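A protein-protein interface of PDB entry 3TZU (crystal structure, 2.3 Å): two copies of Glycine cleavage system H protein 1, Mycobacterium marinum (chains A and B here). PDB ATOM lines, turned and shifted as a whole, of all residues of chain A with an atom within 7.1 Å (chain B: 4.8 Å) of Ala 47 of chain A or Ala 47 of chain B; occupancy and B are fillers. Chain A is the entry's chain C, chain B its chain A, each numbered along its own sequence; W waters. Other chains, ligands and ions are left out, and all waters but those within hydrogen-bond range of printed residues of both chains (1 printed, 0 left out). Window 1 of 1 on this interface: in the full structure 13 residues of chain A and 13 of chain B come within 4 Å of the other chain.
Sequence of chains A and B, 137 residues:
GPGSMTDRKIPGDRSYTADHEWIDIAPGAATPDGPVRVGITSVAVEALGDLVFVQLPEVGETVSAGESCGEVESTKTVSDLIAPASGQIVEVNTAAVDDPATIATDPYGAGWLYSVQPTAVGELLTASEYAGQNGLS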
ATOM      1  N   ALA A  18      30.441 -19.879   9.062  1.00  0.00           N
ATOM      2  CA  ALA A  18      29.061 -20.331   9.331  1.00  0.00           C
ATOM      3  C   ALA A  18      28.012 -19.744   8.361  1.00  0.00           C
ATOM      4  O   ALA A  18      26.889 -20.281   8.255  1.00  0.00           O
ATOM      5  CB  ALA A  18      28.692 -20.037  10.805  1.00  0.00           C
ATOM      6  N   ASP A  19      28.383 -18.665   7.654  1.00  0.00           N
ATOM      7  CA  ASP A  19      27.542 -18.058   6.596  1.00  0.00           C
ATOM      8  C   ASP A  19      27.745 -18.629   5.189  1.00  0.00           C
ATOM      9  O   ASP A  19      27.288 -18.046   4.200  1.00  0.00           O
ATOM     10  CB  ASP A  19      27.807 -16.532   6.551  1.00  0.00           C
ATOM     11  CG  ASP A  19      27.233 -15.826   7.750  1.00  0.00           C
ATOM     12  OD1 ASP A  19      26.078 -16.160   8.064  1.00  0.00           O
ATOM     13  OD2 ASP A  19      27.898 -14.981   8.390  1.00  0.00           O
ATOM     14  N   HIS A  20      28.459 -19.743   5.079  1.00  0.00           N
ATOM     15  CA  HIS A  20      28.617 -20.427   3.790  1.00  0.00           C
ATOM     16  C   HIS A  20      29.447 -19.675   2.804  1.00  0.00           C
ATOM     17  O   HIS A  20      29.152 -19.648   1.595  1.00  0.00           O
ATOM     18  CB  HIS A  20      27.245 -20.783   3.246  1.00  0.00           C
ATOM     19  CG  HIS A  20      26.377 -21.413   4.279  1.00  0.00           C
ATOM     20  ND1 HIS A  20      26.659 -22.618   4.804  1.00  0.00           N
ATOM     21  CD2 HIS A  20      25.272 -20.933   4.957  1.00  0.00           C
ATOM     22  CE1 HIS A  20      25.757 -22.922   5.745  1.00  0.00           C
ATOM     23  NE2 HIS A  20      24.889 -21.889   5.830  1.00  0.00           N
ATOM     24  N   SER A  42      29.469 -24.829  -1.775  1.00  0.00           N
ATOM     25  CA  SER A  42      28.525 -25.567  -2.546  1.00  0.00           C
ATOM     26  C   SER A  42      27.209 -25.659  -1.772  1.00  0.00           C
ATOM     27  O   SER A  42      26.166 -25.889  -2.365  1.00  0.00           O
ATOM     28  CB  SER A  42      29.044 -26.966  -2.773  1.00  0.00           C
ATOM     29  OG  SER A  42      29.481 -27.494  -1.531  1.00  0.00           O
ATOM     30  N   VAL A  43      27.263 -25.508  -0.450  1.00  0.00           N
ATOM     31  CA  VAL A  43      26.043 -25.509   0.316  1.00  0.00           C
ATOM     32  C   VAL A  43      25.284 -24.267  -0.029  1.00  0.00           C
ATOM     33  O   VAL A  43      24.047 -24.327  -0.253  1.00  0.00           O
ATOM     34  CB  VAL A  43      26.282 -25.643   1.835  1.00  0.00           C
ATOM     35  CG1 VAL A  43      24.942 -25.552   2.560  1.00  0.00           C
ATOM     36  CG2 VAL A  43      27.018 -26.969   2.127  1.00  0.00           C
ATOM     37  N   ALA A  44      26.004 -23.149  -0.146  1.00  0.00           N
ATOM     38  CA  ALA A  44      25.352 -21.914  -0.533  1.00  0.00           C
ATOM     39  C   ALA A  44      24.646 -22.023  -1.888  1.00  0.00           C
ATOM     40  O   ALA A  44      23.530 -21.592  -2.033  1.00  0.00           O
ATOM     41  CB  ALA A  44      26.292 -20.750  -0.519  1.00  0.00           C
ATOM     42  N   VAL A  45      25.319 -22.602  -2.869  1.00  0.00           N
ATOM     43  CA  VAL A  45      24.760 -22.753  -4.214  1.00  0.00           C
ATOM     44  C   VAL A  45      23.489 -23.600  -4.204  1.00  0.00           C
ATOM     45  O   VAL A  45      22.489 -23.195  -4.791  1.00  0.00           O
ATOM     46  CB  VAL A  45      25.784 -23.386  -5.192  1.00  0.00           C
ATOM     47  CG1 VAL A  45      25.113 -23.787  -6.506  1.00  0.00           C
ATOM     48  CG2 VAL A  45      26.930 -22.417  -5.438  1.00  0.00           C
ATOM     49  N   GLU A  46      23.557 -24.768  -3.578  1.00  0.00           N
ATOM     50  CA  GLU A  46      22.412 -25.691  -3.443  1.00  0.00           C
ATOM     51  C   GLU A  46      21.167 -24.959  -2.919  1.00  0.00           C
ATOM     52  O   GLU A  46      20.100 -25.051  -3.508  1.00  0.00           O
ATOM     53  CB  GLU A  46      22.779 -26.921  -2.577  1.00  0.00           C
ATOM     54  CG  GLU A  46      23.544 -27.955  -3.391  1.00  0.00           C
ATOM     55  CD  GLU A  46      24.306 -29.051  -2.600  1.00  0.00           C
ATOM     56  OE1 GLU A  46      24.195 -29.157  -1.336  1.00  0.00           O
ATOM     57  OE2 GLU A  46      25.010 -29.854  -3.283  1.00  0.00           O
ATOM     58  N   ALA A  47      21.372 -24.178  -1.865  1.00  0.00           N
ATOM     59  CA  ALA A  47      20.352 -23.374  -1.215  1.00  0.00           C
ATOM     60  C   ALA A  47      19.832 -22.280  -2.095  1.00  0.00           C
ATOM     61  O   ALA A  47      18.621 -22.166  -2.253  1.00  0.00           O
ATOM     62  CB  ALA A  47      20.874 -22.755   0.080  1.00  0.00           C
ATOM     63  N   LEU A  48      20.716 -21.469  -2.659  1.00  0.00           N
ATOM     64  CA  LEU A  48      20.246 -20.355  -3.489  1.00  0.00           C
ATOM     65  C   LEU A  48      19.442 -20.750  -4.739  1.00  0.00           C
ATOM     66  O   LEU A  48      18.496 -20.077  -5.073  1.00  0.00           O
ATOM     67  CB  LEU A  48      21.406 -19.452  -3.919  1.00  0.00           C
ATOM     68  CG  LEU A  48      22.040 -18.695  -2.756  1.00  0.00           C
ATOM     69  CD1 LEU A  48      23.481 -18.311  -3.086  1.00  0.00           C
ATOM     70  CD2 LEU A  48      21.181 -17.478  -2.455  1.00  0.00           C
ATOM     71  N   GLY A  49      19.859 -21.798  -5.443  1.00  0.00           N
ATOM     72  CA  GLY A  49      19.324 -22.108  -6.778  1.00  0.00           C
ATOM     73  C   GLY A  49      20.175 -21.526  -7.899  1.00  0.00           C
ATOM     74  O   GLY A  49      21.332 -21.151  -7.681  1.00  0.00           O
ATOM     75  N   ASP A  50      19.620 -21.435  -9.103  1.00  0.00           N
ATOM     76  CA  ASP A  50      20.366 -20.831 -10.210  1.00  0.00           C
ATOM     77  C   ASP A  50      20.627 -19.342  -9.922  1.00  0.00           C
ATOM     78  O   ASP A  50      19.692 -18.578  -9.736  1.00  0.00           O
ATOM     79  CB  ASP A  50      19.606 -20.986 -11.549  1.00  0.00           C
ATOM     80  CG  ASP A  50      19.573 -22.437 -12.060  1.00  0.00           C
ATOM     81  OD1 ASP A  50      20.588 -23.165 -11.905  1.00  0.00           O
ATOM     82  OD2 ASP A  50      18.522 -22.836 -12.641  1.00  0.00           O
ATOM     83  N   SER A  74      19.574 -15.393  -6.701  1.00  0.00           N
ATOM     84  CA  SER A  74      18.843 -16.277  -7.634  1.00  0.00           C
ATOM     85  C   SER A  74      17.473 -15.699  -7.898  1.00  0.00           C
ATOM     86  O   SER A  74      17.102 -14.686  -7.341  1.00  0.00           O
ATOM     87  CB  SER A  74      18.629 -17.640  -6.995  1.00  0.00           C
ATOM     88  OG  SER A  74      17.849 -17.515  -5.820  1.00  0.00           O
ATOM     89  N   LYS A  76      14.803 -16.778  -6.733  1.00  0.00           N
ATOM     90  CA  LYS A  76      13.979 -16.867  -5.528  1.00  0.00           C
ATOM     91  C   LYS A  76      14.642 -16.348  -4.223  1.00  0.00           C
ATOM     92  O   LYS A  76      13.972 -16.240  -3.189  1.00  0.00           O
ATOM     93  CB  LYS A  76      13.486 -18.313  -5.343  1.00  0.00           C
ATOM     94  CG  LYS A  76      14.529 -19.289  -4.809  1.00  0.00           C
ATOM     95  CD  LYS A  76      14.294 -20.751  -5.231  1.00  0.00           C
ATOM     96  CE  LYS A  76      15.587 -21.588  -5.109  1.00  0.00           C
ATOM     97  NZ  LYS A  76      16.047 -21.826  -3.698  1.00  0.00           N
ATOM     98  N   THR A  77      15.918 -15.970  -4.270  1.00  0.00           N
ATOM     99  CA  THR A  77      16.615 -15.607  -3.063  1.00  0.00           C
ATOM    100  C   THR A  77      17.679 -14.505  -3.266  1.00  0.00           C
ATOM    101  O   THR A  77      18.426 -14.511  -4.249  1.00  0.00           O
ATOM    102  CB  THR A  77      17.285 -16.880  -2.465  1.00  0.00           C
ATOM    103  OG1 THR A  77      16.285 -17.889  -2.232  1.00  0.00           O
ATOM    104  CG2 THR A  77      18.031 -16.571  -1.144  1.00  0.00           C
ATOM    105  N   SER A  79      20.805 -12.756  -0.938  1.00  0.00           N
ATOM    106  CA  SER A  79      21.632 -13.216   0.159  1.00  0.00           C
ATOM    107  C   SER A  79      22.896 -12.368   0.259  1.00  0.00           C
ATOM    108  O   SER A  79      23.651 -12.220  -0.714  1.00  0.00           O
ATOM    109  CB  SER A  79      21.983 -14.674  -0.098  1.00  0.00           C
ATOM    110  OG  SER A  79      22.536 -15.253   1.063  1.00  0.00           O
ATOM    111  N   ASN A 134      26.609 -28.823   8.765  1.00  0.00           N
ATOM    112  CA  ASN A 134      25.662 -28.966   7.674  1.00  0.00           C
ATOM    113  C   ASN A 134      25.331 -30.409   7.350  1.00  0.00           C
ATOM    114  O   ASN A 134      24.806 -30.675   6.266  1.00  0.00           O
ATOM    115  CB  ASN A 134      26.216 -28.280   6.442  1.00  0.00           C
ATOM    116  CG  ASN A 134      26.326 -26.799   6.638  1.00  0.00           C
ATOM    117  OD1 ASN A 134      25.334 -26.081   6.595  1.00  0.00           O
ATOM    118  ND2 ASN A 134      27.514 -26.350   6.933  1.00  0.00           N
ATOM    119  N   HIS B  20      13.506 -26.539  -1.237  1.00  0.00           N
ATOM    120  CA  HIS B  20      13.733 -26.692   0.205  1.00  0.00           C
ATOM    121  C   HIS B  20      12.528 -26.493   1.084  1.00  0.00           C
ATOM    122  O   HIS B  20      12.632 -25.983   2.201  1.00  0.00           O
ATOM    123  CB  HIS B  20      14.898 -25.823   0.670  1.00  0.00           C
ATOM    124  CG  HIS B  20      16.153 -26.055  -0.100  1.00  0.00           C
ATOM    125  ND1 HIS B  20      16.818 -27.202  -0.035  1.00  0.00           N
ATOM    126  CD2 HIS B  20      16.816 -25.262  -1.034  1.00  0.00           C
ATOM    127  CE1 HIS B  20      17.879 -27.147  -0.866  1.00  0.00           C
ATOM    128  NE2 HIS B  20      17.870 -25.952  -1.470  1.00  0.00           N
ATOM    129  N   VAL B  43      17.604 -28.103   5.958  1.00  0.00           N
ATOM    130  CA  VAL B  43      18.641 -27.581   5.103  1.00  0.00           C
ATOM    131  C   VAL B  43      18.359 -26.119   4.847  1.00  0.00           C
ATOM    132  O   VAL B  43      19.267 -25.319   4.811  1.00  0.00           O
ATOM    133  CB  VAL B  43      18.707 -28.356   3.768  1.00  0.00           C
ATOM    134  CG1 VAL B  43      19.722 -27.700   2.817  1.00  0.00           C
ATOM    135  CG2 VAL B  43      19.043 -29.834   4.026  1.00  0.00           C
ATOM    136  N   ALA B  44      17.095 -25.735   4.718  1.00  0.00           N
ATOM    137  CA  ALA B  44      16.820 -24.314   4.464  1.00  0.00           C
ATOM    138  C   ALA B  44      17.189 -23.490   5.707  1.00  0.00           C
ATOM    139  O   ALA B  44      17.810 -22.428   5.610  1.00  0.00           O
ATOM    140  CB  ALA B  44      15.412 -24.089   4.036  1.00  0.00           C
ATOM    141  N   VAL B  45      16.855 -24.023   6.876  1.00  0.00           N
ATOM    142  CA  VAL B  45      17.161 -23.382   8.124  1.00  0.00           C
ATOM    143  C   VAL B  45      18.672 -23.103   8.180  1.00  0.00           C
ATOM    144  O   VAL B  45      19.081 -21.981   8.446  1.00  0.00           O
ATOM    145  CB  VAL B  45      16.704 -24.266   9.312  1.00  0.00           C
ATOM    146  CG1 VAL B  45      17.296 -23.770  10.624  1.00  0.00           C
ATOM    147  CG2 VAL B  45      15.165 -24.308   9.349  1.00  0.00           C
ATOM    148  N   GLU B  46      19.492 -24.114   7.900  1.00  0.00           N
ATOM    149  CA  GLU B  46      20.951 -23.916   7.995  1.00  0.00           C
ATOM    150  C   GLU B  46      21.468 -22.996   6.895  1.00  0.00           C
ATOM    151  O   GLU B  46      22.389 -22.214   7.133  1.00  0.00           O
ATOM    152  CB  GLU B  46      21.709 -25.239   8.047  1.00  0.00           C
ATOM    153  CG  GLU B  46      22.285 -25.528   9.431  1.00  0.00           C
ATOM    154  CD  GLU B  46      23.593 -24.794   9.705  1.00  0.00           C
ATOM    155  OE1 GLU B  46      23.980 -24.720  10.888  1.00  0.00           O
ATOM    156  OE2 GLU B  46      24.252 -24.306   8.753  1.00  0.00           O
ATOM    157  N   ALA B  47      20.852 -23.031   5.731  1.00  0.00           N
ATOM    158  CA  ALA B  47      21.131 -22.073   4.678  1.00  0.00           C
ATOM    159  C   ALA B  47      20.885 -20.599   5.154  1.00  0.00           C
ATOM    160  O   ALA B  47      21.758 -19.755   5.036  1.00  0.00           O
ATOM    161  CB  ALA B  47      20.280 -22.389   3.441  1.00  0.00           C
ATOM    162  N   LEU B  48      19.727 -20.342   5.747  1.00  0.00           N
ATOM    163  CA  LEU B  48      19.265 -18.982   6.041  1.00  0.00           C
ATOM    164  C   LEU B  48      19.972 -18.295   7.223  1.00  0.00           C
ATOM    165  O   LEU B  48      20.241 -17.092   7.198  1.00  0.00           O
ATOM    166  CB  LEU B  48      17.738 -19.039   6.307  1.00  0.00           C
ATOM    167  CG  LEU B  48      16.917 -19.265   5.025  1.00  0.00           C
ATOM    168  CD1 LEU B  48      15.690 -20.152   5.249  1.00  0.00           C
ATOM    169  CD2 LEU B  48      16.527 -17.899   4.464  1.00  0.00           C
ATOM    170  N   GLY B  49      20.230 -19.076   8.267  1.00  0.00           N
ATOM    171  CA  GLY B  49      20.688 -18.538   9.547  1.00  0.00           C
ATOM    172  C   GLY B  49      19.532 -18.223  10.474  1.00  0.00           C
ATOM    173  O   GLY B  49      18.481 -18.834  10.409  1.00  0.00           O
ATOM    174  N   LYS B  76      20.545 -12.050   7.045  1.00  0.00           N
ATOM    175  CA  LYS B  76      21.379 -11.941   5.834  1.00  0.00           C
ATOM    176  C   LYS B  76      20.703 -12.370   4.520  1.00  0.00           C
ATOM    177  O   LYS B  76      21.237 -12.115   3.467  1.00  0.00           O
ATOM    178  CB  LYS B  76      22.645 -12.771   6.023  1.00  0.00           C
ATOM    179  CG  LYS B  76      22.371 -14.276   6.061  1.00  0.00           C
ATOM    180  CD  LYS B  76      23.652 -15.128   6.017  1.00  0.00           C
ATOM    181  CE  LYS B  76      23.363 -16.586   5.537  1.00  0.00           C
ATOM    182  NZ  LYS B  76      24.087 -16.899   4.254  1.00  0.00           N
HETATM  183  O   HOH W   1      23.856 -19.747   8.396  1.00  0.00           O
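A ring nitrogen (NE2) of His 20 of chain B lies within hydrogen-bond range of the backbone carbonyl oxygen (O) of Glu 46 of chain A. OE2 of Glu 46 of chain B lies close to OD1 of Asn 134 of chain A, at 3.0 Å. O of Glu 46 of chain B is in hydrogen-bond range of NE2 of His 20 of chain A. The side-chain amino group of Lys 76 of chain B sits at hydrogen-bond distance from the backbone carbonyl oxygen of Asp 19 of chain A.
NZ of Lys 76 of chain A is in hydrogen-bond range of O of Ala 47 of chain A (3.0 Å).
O of Ala 47 of chain B touches CD2 of His 20 of chain A, 3.7 Å away. His 20 of chain B touches Ala 47 of chain A (NE2 to CA, 3.6 Å). Ala 47 of chain A touches Ala 47 of chain B (CB to CB, 3.4 Å). Lys 76 of chain B touches Ser 79 of chain A.
Of the printed residues of chain B, Asp 19 of chain A touches Lys 76 (3.3 Å). Printed residues of chain B within 4 Å of Glu 46 of chain A: His 20 (3.2 Å). Ala 47 of chain A touches just these residues of chain B: His 20 and Ala 47. Of the printed residues of chain A, His 20 of chain B touches Glu 46 (3.2 Å) and Ala 47 (3.6 Å). Printed residues of chain A within 4 Å of Ala 47 of chain B: His 20 and Ala 47. The nearest residue of chain A that does not touch Ala 47 of chain B is Asn 134 of chain A (5.5 Å). The nearest printed residue of chain B that does not touch Glu 46 of chain A is Val 43 of chain B (6.2 Å).
Of the 17 printed residues of chain A, 6 touch a printed residue of chain B. Printed residues of chain A that touch a printed residue of chain B: Asp 19, His 20, Glu 46, Ala 47, Ser 79 and Asn 134. Along chain A the printed residues that touch a printed residue of chain B span positions 19 to 134. Of the 9 printed residues of chain B, 4 touch a printed residue of chain A.
His 20 of chain A touches Glu 46 of chain B, and with the chains exchanged Glu 46 of chain A touches His 20 of chain B. His 20 of chain A touches Ala 47 of chain B, and with the chains exchanged Ala 47 of chain A touches His 20 of chain B. Ala 47 of chain B touches its own counterpart, Ala 47 of chain A. Positions printed for both chains: 20, 43, 44, 45, 46, 47, 48, 49 and 76.
Water W1 lies within hydrogen-bond range of the backbone carbonyl oxygen (O) of Ala 18 of chain A, the backbone carbonyl oxygen (O) of Glu 46 of chain B and a ring nitrogen (NE2) of His 20 of chain A.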
